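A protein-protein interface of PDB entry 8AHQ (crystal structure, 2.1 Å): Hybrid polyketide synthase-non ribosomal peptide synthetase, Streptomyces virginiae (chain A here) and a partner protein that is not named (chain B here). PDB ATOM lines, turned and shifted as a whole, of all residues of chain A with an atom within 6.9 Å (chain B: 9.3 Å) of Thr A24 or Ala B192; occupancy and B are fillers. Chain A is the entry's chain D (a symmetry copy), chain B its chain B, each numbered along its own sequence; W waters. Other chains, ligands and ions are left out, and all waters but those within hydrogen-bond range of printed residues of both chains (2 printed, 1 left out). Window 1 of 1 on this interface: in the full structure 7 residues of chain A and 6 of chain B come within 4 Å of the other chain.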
ATOM      1  N   GLU A  19     -18.232 -32.116  21.270  1.00  0.00           N
ATOM      2  CA  GLU A  19     -16.843 -32.598  21.036  1.00  0.00           C
ATOM      3  C   GLU A  19     -15.896 -31.408  21.275  1.00  0.00           C
ATOM      4  O   GLU A  19     -14.859 -31.610  21.887  1.00  0.00           O
ATOM      5  CB  GLU A  19     -16.700 -33.271  19.673  1.00  0.00           C
ATOM      6  CG  GLU A  19     -17.320 -34.669  19.675  1.00  0.00           C
ATOM      7  CD  GLU A  19     -17.687 -35.276  18.325  1.00  0.00           C
ATOM      8  OE1 GLU A  19     -17.264 -34.701  17.276  1.00  0.00           O
ATOM      9  OE2 GLU A  19     -18.393 -36.331  18.321  1.00  0.00           O
ATOM     10  N   GLU A  20     -16.253 -30.193  20.869  1.00  0.00           N
ATOM     11  CA  GLU A  20     -15.301 -29.072  20.980  1.00  0.00           C
ATOM     12  C   GLU A  20     -15.127 -28.726  22.481  1.00  0.00           C
ATOM     13  O   GLU A  20     -14.006 -28.453  22.884  1.00  0.00           O
ATOM     14  CB  GLU A  20     -15.794 -27.894  20.137  1.00  0.00           C
ATOM     15  CG  GLU A  20     -14.954 -26.641  20.304  1.00  0.00           C
ATOM     16  CD  GLU A  20     -13.541 -26.768  19.768  1.00  0.00           C
ATOM     17  OE1 GLU A  20     -13.233 -27.820  19.131  1.00  0.00           O
ATOM     18  OE2 GLU A  20     -12.764 -25.821  19.988  1.00  0.00           O
ATOM     19  N   LEU A  21     -16.228 -28.720  23.237  1.00  0.00           N
ATOM     20  CA  LEU A  21     -16.299 -28.440  24.689  1.00  0.00           C
ATOM     21  C   LEU A  21     -15.437 -29.466  25.413  1.00  0.00           C
ATOM     22  O   LEU A  21     -14.577 -29.052  26.183  1.00  0.00           O
ATOM     23  CB  LEU A  21     -17.760 -28.454  25.153  1.00  0.00           C
ATOM     24  CG  LEU A  21     -17.990 -27.812  26.529  1.00  0.00           C
ATOM     25  CD1 LEU A  21     -17.390 -26.414  26.581  1.00  0.00           C
ATOM     26  CD2 LEU A  21     -19.479 -27.750  26.878  1.00  0.00           C
ATOM     27  N   ALA A  22     -15.613 -30.751  25.109  1.00  0.00           N
ATOM     28  CA  ALA A  22     -14.778 -31.865  25.620  1.00  0.00           C
ATOM     29  C   ALA A  22     -13.285 -31.548  25.411  1.00  0.00           C
ATOM     30  O   ALA A  22     -12.490 -31.634  26.379  1.00  0.00           O
ATOM     31  CB  ALA A  22     -15.193 -33.158  24.950  1.00  0.00           C
ATOM     32  N   ARG A  23     -12.868 -31.184  24.202  1.00  0.00           N
ATOM     33  CA  ARG A  23     -11.447 -30.820  23.971  1.00  0.00           C
ATOM     34  C   ARG A  23     -11.046 -29.593  24.801  1.00  0.00           C
ATOM     35  O   ARG A  23      -9.949 -29.625  25.336  1.00  0.00           O
ATOM     36  CB  ARG A  23     -11.161 -30.561  22.498  1.00  0.00           C
ATOM     37  CG  ARG A  23     -11.299 -31.783  21.605  1.00  0.00           C
ATOM     38  CD  ARG A  23     -10.767 -31.430  20.226  1.00  0.00           C
ATOM     39  NE  ARG A  23     -11.791 -30.764  19.444  1.00  0.00           N
ATOM     40  CZ  ARG A  23     -12.731 -31.386  18.710  1.00  0.00           C
ATOM     41  NH1 ARG A  23     -12.808 -32.711  18.684  1.00  0.00           N
ATOM     42  NH2 ARG A  23     -13.611 -30.658  18.034  1.00  0.00           N
ATOM     43  N   THR A  24     -11.855 -28.537  24.900  1.00  0.00           N
ATOM     44  CA  THR A  24     -11.445 -27.297  25.622  1.00  0.00           C
ATOM     45  C   THR A  24     -11.244 -27.622  27.123  1.00  0.00           C
ATOM     46  O   THR A  24     -10.386 -26.983  27.757  1.00  0.00           O
ATOM     47  CB  THR A  24     -12.485 -26.180  25.423  1.00  0.00           C
ATOM     48  OG1 THR A  24     -12.708 -26.033  24.008  1.00  0.00           O
ATOM     49  CG2 THR A  24     -12.049 -24.864  26.022  1.00  0.00           C
ATOM     50  N   LEU A  25     -12.063 -28.525  27.670  1.00  0.00           N
ATOM     51  CA  LEU A  25     -12.122 -28.852  29.123  1.00  0.00           C
ATOM     52  C   LEU A  25     -11.391 -30.154  29.467  1.00  0.00           C
ATOM     53  O   LEU A  25     -11.373 -30.481  30.645  1.00  0.00           O
ATOM     54  CB  LEU A  25     -13.572 -28.929  29.585  1.00  0.00           C
ATOM     55  CG  LEU A  25     -14.426 -27.705  29.314  1.00  0.00           C
ATOM     56  CD1 LEU A  25     -15.849 -27.976  29.774  1.00  0.00           C
ATOM     57  CD2 LEU A  25     -13.876 -26.470  30.022  1.00  0.00           C
ATOM     58  N   TYR A  26     -10.735 -30.826  28.519  1.00  0.00           N
ATOM     59  CA  TYR A  26      -9.819 -31.967  28.784  1.00  0.00           C
ATOM     60  C   TYR A  26     -10.665 -33.079  29.409  1.00  0.00           C
ATOM     61  O   TYR A  26     -10.320 -33.642  30.453  1.00  0.00           O
ATOM     62  CB  TYR A  26      -8.597 -31.506  29.602  1.00  0.00           C
ATOM     63  CG  TYR A  26      -7.543 -30.811  28.764  1.00  0.00           C
ATOM     64  CD1 TYR A  26      -6.544 -31.547  28.150  1.00  0.00           C
ATOM     65  CD2 TYR A  26      -7.587 -29.436  28.505  1.00  0.00           C
ATOM     66  CE1 TYR A  26      -5.587 -30.946  27.357  1.00  0.00           C
ATOM     67  CE2 TYR A  26      -6.659 -28.820  27.674  1.00  0.00           C
ATOM     68  CZ  TYR A  26      -5.642 -29.589  27.099  1.00  0.00           C
ATOM     69  OH  TYR A  26      -4.691 -29.051  26.278  1.00  0.00           O
ATOM     70  N   CYS A  27     -11.821 -33.338  28.812  1.00  0.00           N
ATOM     71  CA  CYS A  27     -12.668 -34.505  29.169  1.00  0.00           C
ATOM     72  C   CYS A  27     -13.179 -35.182  27.891  1.00  0.00           C
ATOM     73  O   CYS A  27     -12.846 -34.705  26.788  1.00  0.00           O
ATOM     74  CB  CYS A  27     -13.811 -34.087  30.082  1.00  0.00           C
ATOM     75  SG  CYS A  27     -15.070 -33.130  29.212  1.00  0.00           S
ATOM     76  N   GLY A  42     -17.272 -25.735  34.026  1.00  0.00           N
ATOM     77  CA  GLY A  42     -15.993 -25.033  34.308  1.00  0.00           C
ATOM     78  C   GLY A  42     -15.467 -24.271  33.090  1.00  0.00           C
ATOM     79  O   GLY A  42     -14.224 -24.122  32.963  1.00  0.00           O
ATOM     80  N   LEU A  43     -16.368 -23.746  32.252  1.00  0.00           N
ATOM     81  CA  LEU A  43     -15.958 -22.907  31.092  1.00  0.00           C
ATOM     82  C   LEU A  43     -15.908 -21.438  31.527  1.00  0.00           C
ATOM     83  O   LEU A  43     -16.966 -20.902  31.840  1.00  0.00           O
ATOM     84  CB  LEU A  43     -16.947 -23.123  29.946  1.00  0.00           C
ATOM     85  CG  LEU A  43     -16.605 -22.449  28.620  1.00  0.00           C
ATOM     86  CD1 LEU A  43     -15.530 -23.224  27.885  1.00  0.00           C
ATOM     87  CD2 LEU A  43     -17.843 -22.326  27.749  1.00  0.00           C
ATOM     88  N   ASP A  44     -14.726 -20.822  31.517  1.00  0.00           N
ATOM     89  CA  ASP A  44     -14.529 -19.417  31.982  1.00  0.00           C
ATOM     90  C   ASP A  44     -14.855 -18.398  30.872  1.00  0.00           C
ATOM     91  O   ASP A  44     -15.207 -18.859  29.777  1.00  0.00           O
ATOM     92  CB  ASP A  44     -13.126 -19.275  32.581  1.00  0.00           C
ATOM     93  CG  ASP A  44     -12.022 -19.020  31.578  1.00  0.00           C
ATOM     94  OD1 ASP A  44     -12.041 -19.653  30.523  1.00  0.00           O
ATOM     95  OD2 ASP A  44     -11.150 -18.191  31.877  1.00  0.00           O
ATOM     96  N   LEU A  47     -12.226 -19.156  27.607  1.00  0.00           N
ATOM     97  CA  LEU A  47     -12.511 -20.290  26.696  1.00  0.00           C
ATOM     98  C   LEU A  47     -13.920 -20.091  26.135  1.00  0.00           C
ATOM     99  O   LEU A  47     -14.176 -20.617  25.051  1.00  0.00           O
ATOM    100  CB  LEU A  47     -12.345 -21.591  27.482  1.00  0.00           C
ATOM    101  CG  LEU A  47     -11.020 -21.739  28.227  1.00  0.00           C
ATOM    102  CD1 LEU A  47     -11.049 -22.947  29.149  1.00  0.00           C
ATOM    103  CD2 LEU A  47      -9.852 -21.829  27.257  1.00  0.00           C
ATOM    104  N   GLY A  48     -14.802 -19.397  26.861  1.00  0.00           N
ATOM    105  CA  GLY A  48     -16.143 -19.009  26.359  1.00  0.00           C
ATOM    106  C   GLY A  48     -16.027 -18.225  25.067  1.00  0.00           C
ATOM    107  O   GLY A  48     -16.706 -18.614  24.093  1.00  0.00           O
ATOM    108  N   GLU A  50     -13.347 -18.154  23.027  1.00  0.00           N
ATOM    109  CA  GLU A  50     -12.836 -19.127  22.018  1.00  0.00           C
ATOM    110  C   GLU A  50     -13.970 -20.040  21.542  1.00  0.00           C
ATOM    111  O   GLU A  50     -14.047 -20.297  20.331  1.00  0.00           O
ATOM    112  CB  GLU A  50     -11.704 -20.001  22.552  1.00  0.00           C
ATOM    113  CG  GLU A  50     -10.451 -19.198  22.825  1.00  0.00           C
ATOM    114  CD  GLU A  50      -9.707 -18.696  21.598  1.00  0.00           C
ATOM    115  OE1 GLU A  50     -10.075 -19.101  20.462  1.00  0.00           O
ATOM    116  OE2 GLU A  50      -8.731 -17.919  21.786  1.00  0.00           O
ATOM    117  N   PHE A  51     -14.822 -20.522  22.445  1.00  0.00           N
ATOM    118  CA  PHE A  51     -15.902 -21.470  22.080  1.00  0.00           C
ATOM    119  C   PHE A  51     -16.878 -20.791  21.102  1.00  0.00           C
ATOM    120  O   PHE A  51     -17.299 -21.474  20.144  1.00  0.00           O
ATOM    121  CB  PHE A  51     -16.656 -21.953  23.312  1.00  0.00           C
ATOM    122  CG  PHE A  51     -17.564 -23.139  23.103  1.00  0.00           C
ATOM    123  CD1 PHE A  51     -17.115 -24.295  22.492  1.00  0.00           C
ATOM    124  CD2 PHE A  51     -18.841 -23.146  23.650  1.00  0.00           C
ATOM    125  CE1 PHE A  51     -17.954 -25.397  22.345  1.00  0.00           C
ATOM    126  CE2 PHE A  51     -19.683 -24.247  23.503  1.00  0.00           C
ATOM    127  CZ  PHE A  51     -19.236 -25.372  22.845  1.00  0.00           C
ATOM    128  N   ARG B  11      -3.483 -34.069  24.551  1.00  0.00           N
ATOM    129  CA  ARG B  11      -3.647 -32.798  23.786  1.00  0.00           C
ATOM    130  C   ARG B  11      -2.753 -31.721  24.431  1.00  0.00           C
ATOM    131  O   ARG B  11      -3.007 -31.347  25.559  1.00  0.00           O
ATOM    132  CB  ARG B  11      -5.132 -32.415  23.794  1.00  0.00           C
ATOM    133  CG  ARG B  11      -5.571 -31.425  22.721  1.00  0.00           C
ATOM    134  CD  ARG B  11      -6.838 -30.599  23.052  1.00  0.00           C
ATOM    135  NE  ARG B  11      -6.463 -29.361  23.742  1.00  0.00           N
ATOM    136  CZ  ARG B  11      -7.220 -28.268  23.921  1.00  0.00           C
ATOM    137  NH1 ARG B  11      -8.457 -28.203  23.467  1.00  0.00           N
ATOM    138  NH2 ARG B  11      -6.727 -27.223  24.570  1.00  0.00           N
ATOM    139  N   LEU B  13       0.101 -32.060  25.774  1.00  0.00           N
ATOM    140  CA  LEU B  13       0.788 -32.488  27.013  1.00  0.00           C
ATOM    141  C   LEU B  13       1.521 -33.807  26.819  1.00  0.00           C
ATOM    142  O   LEU B  13       1.112 -34.644  25.946  1.00  0.00           O
ATOM    143  CB  LEU B  13      -0.192 -32.581  28.196  1.00  0.00           C
ATOM    144  CG  LEU B  13      -1.199 -33.725  28.141  1.00  0.00           C
ATOM    145  CD1 LEU B  13      -0.610 -35.020  28.697  1.00  0.00           C
ATOM    146  CD2 LEU B  13      -2.457 -33.363  28.889  1.00  0.00           C
ATOM    147  N   ARG B  49       2.810 -28.238  25.649  1.00  0.00           N
ATOM    148  CA  ARG B  49       2.818 -27.079  26.579  1.00  0.00           C
ATOM    149  C   ARG B  49       2.898 -27.555  28.041  1.00  0.00           C
ATOM    150  O   ARG B  49       3.280 -26.750  28.881  1.00  0.00           O
ATOM    151  CB  ARG B  49       1.545 -26.260  26.365  1.00  0.00           C
ATOM    152  CG  ARG B  49       1.370 -25.679  24.970  1.00  0.00           C
ATOM    153  CD  ARG B  49      -0.004 -25.069  24.773  1.00  0.00           C
ATOM    154  NE  ARG B  49      -1.058 -26.061  24.644  1.00  0.00           N
ATOM    155  CZ  ARG B  49      -1.951 -26.350  25.581  1.00  0.00           C
ATOM    156  NH1 ARG B  49      -1.923 -25.717  26.741  1.00  0.00           N
ATOM    157  NH2 ARG B  49      -2.864 -27.275  25.361  1.00  0.00           N
ATOM    158  N   VAL B  50       2.518 -28.802  28.334  1.00  0.00           N
ATOM    159  CA  VAL B  50       2.437 -29.259  29.751  1.00  0.00           C
ATOM    160  C   VAL B  50       3.147 -30.608  29.890  1.00  0.00           C
ATOM    161  O   VAL B  50       3.002 -31.450  28.963  1.00  0.00           O
ATOM    162  CB  VAL B  50       0.968 -29.332  30.211  1.00  0.00           C
ATOM    163  CG1 VAL B  50       0.816 -29.705  31.685  1.00  0.00           C
ATOM    164  CG2 VAL B  50       0.214 -28.071  29.839  1.00  0.00           C
ATOM    165  N   LEU B 186      -8.286 -33.203  39.781  1.00  0.00           N
ATOM    166  CA  LEU B 186      -7.948 -31.752  39.804  1.00  0.00           C
ATOM    167  C   LEU B 186      -7.236 -31.383  38.494  1.00  0.00           C
ATOM    168  O   LEU B 186      -7.216 -30.213  38.150  1.00  0.00           O
ATOM    169  CB  LEU B 186      -7.037 -31.468  41.006  1.00  0.00           C
ATOM    170  CG  LEU B 186      -7.606 -31.750  42.392  1.00  0.00           C
ATOM    171  CD1 LEU B 186      -6.505 -31.691  43.434  1.00  0.00           C
ATOM    172  CD2 LEU B 186      -8.698 -30.757  42.735  1.00  0.00           C
ATOM    173  N   LEU B 187      -6.686 -32.368  37.789  1.00  0.00           N
ATOM    174  CA  LEU B 187      -5.881 -32.099  36.567  1.00  0.00           C
ATOM    175  C   LEU B 187      -6.692 -31.518  35.395  1.00  0.00           C
ATOM    176  O   LEU B 187      -6.233 -30.530  34.863  1.00  0.00           O
ATOM    177  CB  LEU B 187      -5.064 -33.336  36.187  1.00  0.00           C
ATOM    178  CG  LEU B 187      -4.095 -33.196  35.020  1.00  0.00           C
ATOM    179  CD1 LEU B 187      -2.911 -32.326  35.396  1.00  0.00           C
ATOM    180  CD2 LEU B 187      -3.624 -34.559  34.549  1.00  0.00           C
ATOM    181  N   PRO B 188      -7.838 -32.071  34.943  1.00  0.00           N
ATOM    182  CA  PRO B 188      -8.536 -31.493  33.788  1.00  0.00           C
ATOM    183  C   PRO B 188      -8.824 -29.979  33.938  1.00  0.00           C
ATOM    184  O   PRO B 188      -8.534 -29.295  32.999  1.00  0.00           O
ATOM    185  CB  PRO B 188      -9.777 -32.373  33.603  1.00  0.00           C
ATOM    186  CG  PRO B 188      -9.410 -33.674  34.267  1.00  0.00           C
ATOM    187  CD  PRO B 188      -8.521 -33.276  35.423  1.00  0.00           C
ATOM    188  N   PRO B 189      -9.370 -29.416  35.054  1.00  0.00           N
ATOM    189  CA  PRO B 189      -9.511 -27.957  35.137  1.00  0.00           C
ATOM    190  C   PRO B 189      -8.199 -27.163  35.057  1.00  0.00           C
ATOM    191  O   PRO B 189      -8.204 -26.008  34.563  1.00  0.00           O
ATOM    192  CB  PRO B 189     -10.153 -27.712  36.518  1.00  0.00           C
ATOM    193  CG  PRO B 189     -10.899 -28.981  36.806  1.00  0.00           C
ATOM    194  CD  PRO B 189     -10.058 -30.081  36.162  1.00  0.00           C
ATOM    195  N   VAL B 190      -7.112 -27.720  35.590  1.00  0.00           N
ATOM    196  CA  VAL B 190      -5.761 -27.095  35.462  1.00  0.00           C
ATOM    197  C   VAL B 190      -5.362 -27.073  33.984  1.00  0.00           C
ATOM    198  O   VAL B 190      -4.839 -26.036  33.567  1.00  0.00           O
ATOM    199  CB  VAL B 190      -4.706 -27.796  36.321  1.00  0.00           C
ATOM    200  CG1 VAL B 190      -3.284 -27.370  35.957  1.00  0.00           C
ATOM    201  CG2 VAL B 190      -5.014 -27.571  37.806  1.00  0.00           C
ATOM    202  N   LEU B 191      -5.537 -28.186  33.261  1.00  0.00           N
ATOM    203  CA  LEU B 191      -5.194 -28.282  31.796  1.00  0.00           C
ATOM    204  C   LEU B 191      -6.091 -27.334  30.990  1.00  0.00           C
ATOM    205  O   LEU B 191      -5.584 -26.667  30.115  1.00  0.00           O
ATOM    206  CB  LEU B 191      -5.319 -29.720  31.291  1.00  0.00           C
ATOM    207  CG  LEU B 191      -4.374 -30.706  31.988  1.00  0.00           C
ATOM    208  CD1 LEU B 191      -4.684 -32.132  31.539  1.00  0.00           C
ATOM    209  CD2 LEU B 191      -2.909 -30.333  31.716  1.00  0.00           C
ATOM    210  N   ALA B 192      -7.377 -27.288  31.302  1.00  0.00           N
ATOM    211  CA  ALA B 192      -8.336 -26.354  30.668  1.00  0.00           C
ATOM    212  C   ALA B 192      -7.826 -24.932  30.878  1.00  0.00           C
ATOM    213  O   ALA B 192      -7.711 -24.181  29.894  1.00  0.00           O
ATOM    214  CB  ALA B 192      -9.711 -26.586  31.220  1.00  0.00           C
ATOM    215  N   GLY B 193      -7.493 -24.572  32.112  1.00  0.00           N
ATOM    216  CA  GLY B 193      -6.974 -23.215  32.427  1.00  0.00           C
ATOM    217  C   GLY B 193      -5.701 -22.892  31.631  1.00  0.00           C
ATOM    218  O   GLY B 193      -5.556 -21.772  31.084  1.00  0.00           O
ATOM    219  N   LEU B 194      -4.756 -23.832  31.580  1.00  0.00           N
ATOM    220  CA  LEU B 194      -3.451 -23.582  30.891  1.00  0.00           C
ATOM    221  C   LEU B 194      -3.596 -23.423  29.365  1.00  0.00           C
ATOM    222  O   LEU B 194      -2.710 -22.765  28.728  1.00  0.00           O
ATOM    223  CB  LEU B 194      -2.502 -24.733  31.203  1.00  0.00           C
ATOM    224  CG  LEU B 194      -1.957 -24.746  32.637  1.00  0.00           C
ATOM    225  CD1 LEU B 194      -1.295 -26.084  32.939  1.00  0.00           C
ATOM    226  CD2 LEU B 194      -0.961 -23.630  32.845  1.00  0.00           C
ATOM    227  N   GLY B 195      -4.585 -24.075  28.769  1.00  0.00           N
ATOM    228  CA  GLY B 195      -4.948 -23.837  27.366  1.00  0.00           C
ATOM    229  C   GLY B 195      -5.306 -22.389  27.048  1.00  0.00           C
ATOM    230  O   GLY B 195      -5.307 -22.082  25.871  1.00  0.00           O
ATOM    231  N   ARG B 196      -5.639 -21.539  28.031  1.00  0.00           N
ATOM    232  CA  ARG B 196      -5.867 -20.090  27.781  1.00  0.00           C
ATOM    233  C   ARG B 196      -4.544 -19.392  27.478  1.00  0.00           C
ATOM    234  O   ARG B 196      -4.567 -18.326  26.902  1.00  0.00           O
ATOM    235  CB  ARG B 196      -6.439 -19.398  29.033  1.00  0.00           C
ATOM    236  CG  ARG B 196      -7.843 -19.859  29.404  1.00  0.00           C
ATOM    237  CD  ARG B 196      -8.302 -19.417  30.783  1.00  0.00           C
ATOM    238  NE  ARG B 196      -7.350 -19.726  31.842  1.00  0.00           N
ATOM    239  CZ  ARG B 196      -7.524 -19.335  33.092  1.00  0.00           C
ATOM    240  NH1 ARG B 196      -8.636 -18.696  33.407  1.00  0.00           N
ATOM    241  NH2 ARG B 196      -6.616 -19.604  34.017  1.00  0.00           N
ATOM    242  N   THR B 197      -3.413 -19.882  27.986  1.00  0.00           N
ATOM    243  CA  THR B 197      -2.124 -19.221  27.714  1.00  0.00           C
ATOM    244  C   THR B 197      -1.359 -20.110  26.736  1.00  0.00           C
ATOM    245  O   THR B 197      -1.997 -20.940  26.071  1.00  0.00           O
ATOM    246  CB  THR B 197      -1.427 -18.829  29.013  1.00  0.00           C
ATOM    247  OG1 THR B 197      -0.320 -18.021  28.615  1.00  0.00           O
ATOM    248  CG2 THR B 197      -0.968 -20.018  29.826  1.00  0.00           C
HETATM  249  O   HOH W   1      -8.274 -25.314  27.384  1.00  0.00           O
HETATM  250  O   HOH W   2      -3.483 -27.335  28.570  1.00  0.00           O
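The guanidinium group (NH1) of Arg B11 is in hydrogen-bond range of the backbone carbonyl oxygen (O) of Arg A23, 2.8 Å away. O of Arg B11 sits at hydrogen-bond distance from OH of Tyr A26 (2.9 Å). NH2 of Arg B49 lies within hydrogen-bond range of OH of Tyr A26, 2.7 Å away. The side-chain carboxylate of Asp A44 lies within salt-bridge range of the guanidinium group of Arg B196.
NE of Arg B196 sits at hydrogen-bond distance from O of Gly B193, 2.8 Å away. The side-chain carboxylate of Glu A20 lies within salt-bridge range of the guanidinium group of Arg A23. OG1 of Thr A24 is in hydrogen-bond range of O of Glu A20, at 3.0 Å. OD1 of Asp A44 is in hydrogen-bond range of N of Leu A47, 3.0 Å away.
Thr A24 touches Arg B11 (N to NH1, 3.7 Å). O of Thr A24 touches CB of Ala B192, 3.6 Å away. CB of Pro B188 touches O of Leu A25, at 3.9 Å. Leu A25 touches Ala B192 (CA to CB, 3.9 Å). Pro B188 touches Tyr A26. CE2 of Tyr A26 touches O of Leu B191 (3.4 Å). Tyr A26 touches Ala B192. Ala B192 touches Leu A47. CG of Arg B196 touches CD2 of Leu A47, at 3.5 Å.
Thr A24 touches two residues of chain B. Gly A42 touches none of the printed residues of chain B. Of the printed residues of chain B, Leu A47 touches Ala B192 (3.6 Å) and Arg B196 (3.5 Å). Of the printed residues of chain A, Arg B49 touches Tyr A26 (2.7 Å). Of the printed residues of chain A, Pro B188 touches Leu A25 and Tyr A26. Printed residues of chain A within 4 Å of Leu B191: Tyr A26. Of chain A, only Thr A24 (3.6 Å), Leu A25 (3.9 Å), Tyr A26 (3.5 Å) and Leu A47 (3.6 Å) come within 4 Å of Ala B192. The nearest residue of chain B that does not touch Thr A24 is Leu B191 (5.4 Å). The nearest residue of chain A that does not touch Ala B192 is Gly A42 (5.4 Å).
Of the 16 printed residues of chain A, 6 touch a printed residue of chain B. Hydrophobic or aromatic side chains of chain A that line the printed part of chain B: Tyr A26 and Leu A47. Of the 16 printed residues of chain B, 6 touch a printed residue of chain A. Among the printed residues, Asp or Glu carboxylates within 4 Å of a Lys or Arg side-chain nitrogen of the other chain: Asp A44 with Arg B196.
Water W2 lies within hydrogen-bond range of the backbone carbonyl oxygen (O) of Leu B191 (2.7 Å), the guanidinium group (NH1) of Arg B49 (2.9 Å), the side-chain hydroxyl (OH) of Tyr A26 (3.1 Å) and the backbone NH (N) of Gly B195 (3.4 Å). Water W1 bridges the backbone carbonyl oxygen of Thr A24 and the backbone carbonyl oxygen of Ala B192.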
